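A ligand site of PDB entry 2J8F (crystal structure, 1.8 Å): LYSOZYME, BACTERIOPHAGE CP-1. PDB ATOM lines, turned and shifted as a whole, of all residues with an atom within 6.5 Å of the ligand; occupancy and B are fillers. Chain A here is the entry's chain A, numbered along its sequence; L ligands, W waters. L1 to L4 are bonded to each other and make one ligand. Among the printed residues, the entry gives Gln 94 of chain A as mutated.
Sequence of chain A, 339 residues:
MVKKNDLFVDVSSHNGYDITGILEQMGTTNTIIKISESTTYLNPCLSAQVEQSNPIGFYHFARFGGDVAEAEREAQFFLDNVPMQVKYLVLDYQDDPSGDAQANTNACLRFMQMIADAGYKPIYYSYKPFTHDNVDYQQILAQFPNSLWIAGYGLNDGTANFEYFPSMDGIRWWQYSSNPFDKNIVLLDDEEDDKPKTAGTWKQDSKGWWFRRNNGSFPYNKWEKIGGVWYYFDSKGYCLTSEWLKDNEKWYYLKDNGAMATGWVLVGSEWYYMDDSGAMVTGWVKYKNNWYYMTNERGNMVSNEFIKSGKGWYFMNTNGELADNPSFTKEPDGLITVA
O4 of LIG L1 sits at hydrogen-bond distance from OH of Tyr 125 (2.5 Å).
An oxygen (O2) of LIG L1 lies within hydrogen-bond range of the side-chain amide nitrogen of Gln 94 (2.6 Å).
The backbone NH (N) of Tyr 153 sits at hydrogen-bond distance from an oxygen (O7) of LG2 L2, 2.9 Å away.
The backbone carbonyl oxygen of Gly 154 sits at hydrogen-bond distance from a nitrogen (N1) of LG4 L4 (3.0 Å).
The side-chain amide oxygen of Gln 175 lies within hydrogen-bond range of the side-chain hydroxyl of Tyr 125.
The side-chain amide oxygen of Gln 94 lies close to the side-chain carboxylate of Asp 92 (2.7 Å).
OH of Tyr 153 is in hydrogen-bond range of OE1 of Gln 175 (2.6 Å).
N of Ala 151 is in hydrogen-bond range of O of Ser 126 (3.0 Å).
The backbone NH (N) of Gly 152 lies within hydrogen-bond range of the backbone carbonyl oxygen (O) of Gln 175, 3.0 Å away.
Residues that only touch the ligand: Pro 129 (3.0 Å), Leu 155 (3.4 Å), Ala 151 (3.5 Å), Tyr 164 (3.6 Å), Gly 152 (3.6 Å) and Tyr 127 (3.7 Å).
Hydrophobic or aromatic side chains within 4 Å of the ligand: Tyr 125, Tyr 127, Pro 129, Ala 151, Tyr 153, Leu 155 and Tyr 164.
Ten residues have an atom within 4 Å of the ligand: Gln 94, Tyr 125, Tyr 127, Pro 129, Ala 151, Gly 152, Tyr 153, Gly 154, Leu 155 and Tyr 164.
The nearest printed residue that does not touch the ligand is Ser 126 (4.3 Å).
Water W4 lies within hydrogen-bond range of the backbone carbonyl oxygen of Ala 151 (2.6 Å), an oxygen (O6) of LG2 L2 (2.7 Å) and the backbone NH of Lys 128 (3.0 Å).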
ATOM      1  N   PHE A  61     -39.330  -3.411  29.075  1.00  0.00           N
ATOM      2  CA  PHE A  61     -38.423  -4.006  30.070  1.00  0.00           C
ATOM      3  C   PHE A  61     -39.142  -4.090  31.389  1.00  0.00           C
ATOM      4  O   PHE A  61     -39.428  -3.049  32.012  1.00  0.00           O
ATOM      5  CB  PHE A  61     -37.142  -3.186  30.180  1.00  0.00           C
ATOM      6  CG  PHE A  61     -36.035  -3.921  30.923  1.00  0.00           C
ATOM      7  CD1 PHE A  61     -35.114  -4.677  30.262  1.00  0.00           C
ATOM      8  CD2 PHE A  61     -35.979  -3.867  32.302  1.00  0.00           C
ATOM      9  CE1 PHE A  61     -34.111  -5.354  30.970  1.00  0.00           C
ATOM     10  CE2 PHE A  61     -34.975  -4.554  33.007  1.00  0.00           C
ATOM     11  CZ  PHE A  61     -34.062  -5.283  32.361  1.00  0.00           C
ATOM     12  N   ASP A  92     -39.968  -8.300  27.967  1.00  0.00           N
ATOM     13  CA  ASP A  92     -38.552  -8.558  28.196  1.00  0.00           C
ATOM     14  C   ASP A  92     -38.398  -8.762  29.695  1.00  0.00           C
ATOM     15  O   ASP A  92     -38.466  -7.786  30.470  1.00  0.00           O
ATOM     16  CB  ASP A  92     -37.742  -7.354  27.717  1.00  0.00           C
ATOM     17  CG  ASP A  92     -36.241  -7.497  27.921  1.00  0.00           C
ATOM     18  OD1 ASP A  92     -35.771  -8.253  28.798  1.00  0.00           O
ATOM     19  OD2 ASP A  92     -35.470  -6.860  27.199  1.00  0.00           O
ATOM     20  N   GLN A  94     -36.038 -10.307  32.365  1.00  0.00           N
ATOM     21  CA  GLN A  94     -34.672 -10.810  32.611  1.00  0.00           C
ATOM     22  C   GLN A  94     -34.027 -10.229  33.860  1.00  0.00           C
ATOM     23  O   GLN A  94     -32.815 -10.336  34.005  1.00  0.00           O
ATOM     24  CB  GLN A  94     -33.773 -10.494  31.417  1.00  0.00           C
ATOM     25  CG  GLN A  94     -33.527  -8.995  31.182  1.00  0.00           C
ATOM     26  CD  GLN A  94     -32.620  -8.674  30.011  1.00  0.00           C
ATOM     27  OE1 GLN A  94     -33.096  -8.303  28.911  1.00  0.00           O
ATOM     28  NE2 GLN A  94     -31.328  -8.740  30.243  1.00  0.00           N
ATOM     29  N   TYR A 125     -39.574 -12.716  26.199  1.00  0.00           N
ATOM     30  CA  TYR A 125     -38.147 -12.649  25.900  1.00  0.00           C
ATOM     31  C   TYR A 125     -37.355 -12.789  27.182  1.00  0.00           C
ATOM     32  O   TYR A 125     -37.631 -12.091  28.180  1.00  0.00           O
ATOM     33  CB  TYR A 125     -37.758 -11.334  25.222  1.00  0.00           C
ATOM     34  CG  TYR A 125     -36.268 -11.087  25.218  1.00  0.00           C
ATOM     35  CD1 TYR A 125     -35.465 -11.490  24.170  1.00  0.00           C
ATOM     36  CD2 TYR A 125     -35.647 -10.485  26.313  1.00  0.00           C
ATOM     37  CE1 TYR A 125     -34.034 -11.299  24.207  1.00  0.00           C
ATOM     38  CE2 TYR A 125     -34.259 -10.276  26.357  1.00  0.00           C
ATOM     39  CZ  TYR A 125     -33.469 -10.693  25.321  1.00  0.00           C
ATOM     40  OH  TYR A 125     -32.114 -10.496  25.401  1.00  0.00           O
ATOM     41  N   SER A 126     -36.326 -13.639  27.135  1.00  0.00           N
ATOM     42  CA  SER A 126     -35.401 -13.806  28.239  1.00  0.00           C
ATOM     43  C   SER A 126     -34.233 -14.623  27.757  1.00  0.00           C
ATOM     44  O   SER A 126     -34.072 -14.843  26.554  1.00  0.00           O
ATOM     45  CB  SER A 126     -36.101 -14.501  29.440  1.00  0.00           C
ATOM     46  OG  SER A 126     -35.290 -14.436  30.623  1.00  0.00           O
ATOM     47  N   TYR A 127     -33.393 -15.079  28.692  1.00  0.00           N
ATOM     48  CA  TYR A 127     -32.388 -16.096  28.416  1.00  0.00           C
ATOM     49  C   TYR A 127     -32.702 -17.370  29.218  1.00  0.00           C
ATOM     50  O   TYR A 127     -33.463 -17.322  30.165  1.00  0.00           O
ATOM     51  CB  TYR A 127     -30.977 -15.567  28.694  1.00  0.00           C
ATOM     52  CG  TYR A 127     -30.668 -15.050  30.088  1.00  0.00           C
ATOM     53  CD1 TYR A 127     -29.846 -15.777  30.949  1.00  0.00           C
ATOM     54  CD2 TYR A 127     -31.104 -13.785  30.518  1.00  0.00           C
ATOM     55  CE1 TYR A 127     -29.526 -15.298  32.257  1.00  0.00           C
ATOM     56  CE2 TYR A 127     -30.771 -13.292  31.815  1.00  0.00           C
ATOM     57  CZ  TYR A 127     -29.982 -14.071  32.672  1.00  0.00           C
ATOM     58  OH  TYR A 127     -29.662 -13.638  33.923  1.00  0.00           O
ATOM     59  N   LYS A 128     -32.100 -18.509  28.840  1.00  0.00           N
ATOM     60  CA  LYS A 128     -32.473 -19.825  29.296  1.00  0.00           C
ATOM     61  C   LYS A 128     -32.301 -20.089  30.792  1.00  0.00           C
ATOM     62  O   LYS A 128     -33.260 -20.442  31.473  1.00  0.00           O
ATOM     63  CB  LYS A 128     -31.728 -20.870  28.494  1.00  0.00           C
ATOM     64  CG  LYS A 128     -32.123 -22.319  28.790  1.00  0.00           C
ATOM     65  CD  LYS A 128     -31.513 -23.249  27.705  1.00  0.00           C
ATOM     66  CE  LYS A 128     -31.726 -24.732  28.074  1.00  0.00           C
ATOM     67  NZ  LYS A 128     -31.028 -25.638  27.063  1.00  0.00           N
ATOM     68  N   PRO A 129     -31.123 -19.942  31.363  1.00  0.00           N
ATOM     69  CA  PRO A 129     -30.997 -20.214  32.801  1.00  0.00           C
ATOM     70  C   PRO A 129     -31.872 -19.298  33.679  1.00  0.00           C
ATOM     71  O   PRO A 129     -32.416 -19.787  34.684  1.00  0.00           O
ATOM     72  CB  PRO A 129     -29.512 -20.003  33.074  1.00  0.00           C
ATOM     73  CG  PRO A 129     -29.020 -19.340  31.923  1.00  0.00           C
ATOM     74  CD  PRO A 129     -29.817 -19.656  30.743  1.00  0.00           C
ATOM     75  N   PHE A 130     -32.053 -18.041  33.281  1.00  0.00           N
ATOM     76  CA  PHE A 130     -32.943 -17.145  34.001  1.00  0.00           C
ATOM     77  C   PHE A 130     -34.363 -17.660  33.970  1.00  0.00           C
ATOM     78  O   PHE A 130     -35.086 -17.622  34.963  1.00  0.00           O
ATOM     79  CB  PHE A 130     -32.887 -15.725  33.426  1.00  0.00           C
ATOM     80  CG  PHE A 130     -33.723 -14.718  34.203  1.00  0.00           C
ATOM     81  CD1 PHE A 130     -33.158 -13.959  35.212  1.00  0.00           C
ATOM     82  CD2 PHE A 130     -35.058 -14.569  33.930  1.00  0.00           C
ATOM     83  CE1 PHE A 130     -33.906 -13.048  35.940  1.00  0.00           C
ATOM     84  CE2 PHE A 130     -35.850 -13.644  34.636  1.00  0.00           C
ATOM     85  CZ  PHE A 130     -35.286 -12.872  35.634  1.00  0.00           C
ATOM     86  N   ALA A 151     -32.437 -15.556  24.165  1.00  0.00           N
ATOM     87  CA  ALA A 151     -31.071 -15.092  23.921  1.00  0.00           C
ATOM     88  C   ALA A 151     -30.099 -16.175  24.291  1.00  0.00           C
ATOM     89  O   ALA A 151     -30.271 -16.832  25.320  1.00  0.00           O
ATOM     90  CB  ALA A 151     -30.768 -13.839  24.761  1.00  0.00           C
ATOM     91  N   GLY A 152     -29.070 -16.341  23.470  1.00  0.00           N
ATOM     92  CA  GLY A 152     -28.000 -17.302  23.676  1.00  0.00           C
ATOM     93  C   GLY A 152     -26.921 -16.975  22.693  1.00  0.00           C
ATOM     94  O   GLY A 152     -27.121 -17.192  21.507  1.00  0.00           O
ATOM     95  N   TYR A 153     -25.813 -16.418  23.161  1.00  0.00           N
ATOM     96  CA  TYR A 153     -24.822 -15.793  22.289  1.00  0.00           C
ATOM     97  C   TYR A 153     -23.596 -16.627  21.953  1.00  0.00           C
ATOM     98  O   TYR A 153     -22.819 -16.257  21.069  1.00  0.00           O
ATOM     99  CB  TYR A 153     -24.343 -14.437  22.822  1.00  0.00           C
ATOM    100  CG  TYR A 153     -25.403 -13.456  23.216  1.00  0.00           C
ATOM    101  CD1 TYR A 153     -25.143 -12.500  24.146  1.00  0.00           C
ATOM    102  CD2 TYR A 153     -26.696 -13.476  22.622  1.00  0.00           C
ATOM    103  CE1 TYR A 153     -26.118 -11.550  24.511  1.00  0.00           C
ATOM    104  CE2 TYR A 153     -27.655 -12.558  22.992  1.00  0.00           C
ATOM    105  CZ  TYR A 153     -27.375 -11.579  23.920  1.00  0.00           C
ATOM    106  OH  TYR A 153     -28.355 -10.670  24.281  1.00  0.00           O
ATOM    107  N   GLY A 154     -23.465 -17.776  22.590  1.00  0.00           N
ATOM    108  CA  GLY A 154     -22.287 -18.607  22.420  1.00  0.00           C
ATOM    109  C   GLY A 154     -21.074 -17.754  22.772  1.00  0.00           C
ATOM    110  O   GLY A 154     -21.055 -17.171  23.850  1.00  0.00           O
ATOM    111  N   LEU A 155     -20.107 -17.646  21.853  1.00  0.00           N
ATOM    112  CA  LEU A 155     -18.904 -16.846  22.096  1.00  0.00           C
ATOM    113  C   LEU A 155     -19.130 -15.346  21.900  1.00  0.00           C
ATOM    114  O   LEU A 155     -18.255 -14.542  22.232  1.00  0.00           O
ATOM    115  CB  LEU A 155     -17.773 -17.281  21.171  1.00  0.00           C
ATOM    116  CG  LEU A 155     -17.169 -18.683  21.367  1.00  0.00           C
ATOM    117  CD1 LEU A 155     -17.231 -19.131  22.814  1.00  0.00           C
ATOM    118  CD2 LEU A 155     -17.837 -19.681  20.454  1.00  0.00           C
ATOM    119  N   ASN A 156     -20.280 -14.996  21.303  1.00  0.00           N
ATOM    120  CA  ASN A 156     -20.698 -13.616  21.102  1.00  0.00           C
ATOM    121  C   ASN A 156     -19.745 -12.853  20.212  1.00  0.00           C
ATOM    122  O   ASN A 156     -19.262 -11.752  20.542  1.00  0.00           O
ATOM    123  CB  ASN A 156     -20.879 -12.906  22.443  1.00  0.00           C
ATOM    124  CG  ASN A 156     -21.858 -11.782  22.371  1.00  0.00           C
ATOM    125  OD1 ASN A 156     -21.891 -10.954  23.271  1.00  0.00           O
ATOM    126  ND2 ASN A 156     -22.629 -11.697  21.286  1.00  0.00           N
ATOM    127  N   TYR A 164     -24.432 -23.398  20.000  1.00  0.00           N
ATOM    128  CA  TYR A 164     -24.876 -22.765  21.242  1.00  0.00           C
ATOM    129  C   TYR A 164     -26.371 -22.403  21.223  1.00  0.00           C
ATOM    130  O   TYR A 164     -26.835 -21.564  22.023  1.00  0.00           O
ATOM    131  CB  TYR A 164     -24.010 -21.551  21.555  1.00  0.00           C
ATOM    132  CG  TYR A 164     -22.563 -21.881  21.902  1.00  0.00           C
ATOM    133  CD1 TYR A 164     -21.553 -21.822  20.938  1.00  0.00           C
ATOM    134  CD2 TYR A 164     -22.201 -22.181  23.214  1.00  0.00           C
ATOM    135  CE1 TYR A 164     -20.215 -22.105  21.284  1.00  0.00           C
ATOM    136  CE2 TYR A 164     -20.883 -22.466  23.567  1.00  0.00           C
ATOM    137  CZ  TYR A 164     -19.894 -22.420  22.609  1.00  0.00           C
ATOM    138  OH  TYR A 164     -18.601 -22.718  23.004  1.00  0.00           O
ATOM    139  N   GLN A 175     -32.128 -14.630  19.695  1.00  0.00           N
ATOM    140  CA  GLN A 175     -31.181 -13.568  19.784  1.00  0.00           C
ATOM    141  C   GLN A 175     -29.795 -14.171  19.906  1.00  0.00           C
ATOM    142  O   GLN A 175     -29.399 -14.653  20.981  1.00  0.00           O
ATOM    143  CB  GLN A 175     -31.497 -12.633  20.931  1.00  0.00           C
ATOM    144  CG  GLN A 175     -30.777 -11.307  20.896  1.00  0.00           C
ATOM    145  CD  GLN A 175     -31.065 -10.445  22.087  1.00  0.00           C
ATOM    146  OE1 GLN A 175     -30.702 -10.782  23.234  1.00  0.00           O
ATOM    147  NE2 GLN A 175     -31.796  -9.335  21.877  1.00  0.00           N
ATOM    148  N   SER A 178     -25.059 -10.146  20.784  1.00  0.00           N
ATOM    149  CA  SER A 178     -25.169  -8.723  21.103  1.00  0.00           C
ATOM    150  C   SER A 178     -23.985  -7.907  20.579  1.00  0.00           C
ATOM    151  O   SER A 178     -23.895  -6.722  20.812  1.00  0.00           O
ATOM    152  CB  SER A 178     -25.290  -8.545  22.609  1.00  0.00           C
ATOM    153  OG  SER A 178     -24.087  -8.940  23.227  1.00  0.00           O
ATOM    154  N   ASP A 182     -27.683  -6.032  18.959  1.00  0.00           N
ATOM    155  CA  ASP A 182     -28.486  -7.233  19.167  1.00  0.00           C
ATOM    156  C   ASP A 182     -28.966  -7.796  17.839  1.00  0.00           C
ATOM    157  O   ASP A 182     -29.673  -7.093  17.118  1.00  0.00           O
ATOM    158  CB  ASP A 182     -29.723  -6.889  19.993  1.00  0.00           C
ATOM    159  CG  ASP A 182     -29.425  -6.727  21.503  1.00  0.00           C
ATOM    160  OD1 ASP A 182     -28.261  -6.978  21.935  1.00  0.00           O
ATOM    161  OD2 ASP A 182     -30.322  -6.403  22.300  1.00  0.00           O
HETATM  162  C1  LIG L   1     -27.216 -11.723  29.860  1.00  0.00           C
HETATM  163  C2  LIG L   1     -26.607 -10.315  29.664  1.00  0.00           C
HETATM  164  C3  LIG L   1     -27.750  -9.300  29.478  1.00  0.00           C
HETATM  165  C4  LIG L   1     -28.622  -9.695  28.274  1.00  0.00           C
HETATM  166  C5  LIG L   1     -29.185 -11.107  28.525  1.00  0.00           C
HETATM  167  C6  LIG L   1     -30.079 -11.660  27.404  1.00  0.00           C
HETATM  168  C7  LIG L   1     -24.434 -10.135  30.853  1.00  0.00           C
HETATM  169  C8  LIG L   1     -23.710  -9.580  32.096  1.00  0.00           C
HETATM  170  N1  LIG L   1     -25.781 -10.002  30.856  1.00  0.00           N
HETATM  171  O1  LIG L   1     -27.042  -8.177  28.865  1.00  0.00           O
HETATM  172  O2  LIG L   1     -29.706  -8.748  28.190  1.00  0.00           O
HETATM  173  O3  LIG L   1     -28.087 -12.031  28.754  1.00  0.00           O
HETATM  174  O4  LIG L   1     -31.465 -11.351  27.664  1.00  0.00           O
HETATM  175  O5  LIG L   1     -23.823 -10.666  29.937  1.00  0.00           O
HETATM  176  C1  LG2 L   2     -25.376 -16.395  31.709  1.00  0.00           C
HETATM  177  C2  LG2 L   2     -26.019 -16.367  30.290  1.00  0.00           C
HETATM  178  C3  LG2 L   2     -25.789 -15.020  29.588  1.00  0.00           C
HETATM  179  C4  LG2 L   2     -26.374 -13.934  30.494  1.00  0.00           C
HETATM  180  C5  LG2 L   2     -25.684 -13.946  31.863  1.00  0.00           C
HETATM  181  C6  LG2 L   2     -26.221 -12.900  32.842  1.00  0.00           C
HETATM  182  C7  LG2 L   2     -26.470 -18.345  28.863  1.00  0.00           C
HETATM  183  C8  LG2 L   2     -25.854 -19.327  27.852  1.00  0.00           C
HETATM  184  C9  LG2 L   2     -26.349 -14.488  27.193  1.00  0.00           C
HETATM  185  C10 LG2 L   2     -25.207 -15.355  26.589  1.00  0.00           C
HETATM  186  C11 LG2 L   2     -27.661 -14.618  26.393  1.00  0.00           C
HETATM  187  O1  LG2 L   2     -25.729 -17.591  32.373  1.00  0.00           O
HETATM  188  O2  LG2 L   2     -26.760 -14.897  28.527  1.00  0.00           O
HETATM  189  O3  LG2 L   2     -26.128 -12.641  29.915  1.00  0.00           O
HETATM  190  O4  LG2 L   2     -25.823 -15.252  32.467  1.00  0.00           O
HETATM  191  O5  LG2 L   2     -25.494 -12.927  34.087  1.00  0.00           O
HETATM  192  O6  LG2 L   2     -27.672 -18.321  29.091  1.00  0.00           O
HETATM  193  O7  LG2 L   2     -25.446 -16.432  26.058  1.00  0.00           O
HETATM  194  N1  LG2 L   2     -25.596 -17.517  29.481  1.00  0.00           N
HETATM  195  C12 LG2 L   2     -24.799 -17.949  33.380  1.00  0.00           C
HETATM  196  N1  LG3 L   3     -23.915 -14.903  26.678  1.00  0.00           N
HETATM  197  C1  LG3 L   3     -22.718 -15.710  26.351  1.00  0.00           C
HETATM  198  C2  LG3 L   3     -22.539 -17.008  27.194  1.00  0.00           C
HETATM  199  O1  LG3 L   3     -23.092 -17.144  28.274  1.00  0.00           O
HETATM  200  C3  LG3 L   3     -21.492 -14.794  26.330  1.00  0.00           C
HETATM  201  N1  LG4 L   4     -21.720 -17.966  26.683  1.00  0.00           N
HETATM  202  C1  LG4 L   4     -21.375 -19.246  27.335  1.00  0.00           C
HETATM  203  C2  LG4 L   4     -22.355 -20.383  26.955  1.00  0.00           C
HETATM  204  O1  LG4 L   4     -23.175 -20.156  26.022  1.00  0.00           O
HETATM  205  C3  LG4 L   4     -19.923 -19.652  27.021  1.00  0.00           C
HETATM  206  C4  LG4 L   4     -19.233 -18.770  25.968  1.00  0.00           C
HETATM  207  C5  LG4 L   4     -17.733 -18.759  26.178  1.00  0.00           C
HETATM  208  O2  LG4 L   4     -17.086 -19.795  26.223  1.00  0.00           O
HETATM  209  O3  LG4 L   4     -22.262 -21.450  27.625  1.00  0.00           O
HETATM  210  O   HOH W   1     -28.539 -21.118  26.591  1.00  0.00           O
HETATM  211  O   HOH W   2     -26.442 -10.636  35.945  1.00  0.00           O
HETATM  212  O   HOH W   3     -18.146 -14.097  25.832  1.00  0.00           O
HETATM  213  O   HOH W   4     -29.592 -18.550  27.144  1.00  0.00           O
HETATM  214  O   HOH W   5     -23.396 -12.617  28.501  1.00  0.00           O
HETATM  215  O   HOH W   6     -25.529 -20.372  31.570  1.00  0.00           O
HETATM  216  O   HOH W   7     -24.421 -22.536  26.038  1.00  0.00           O
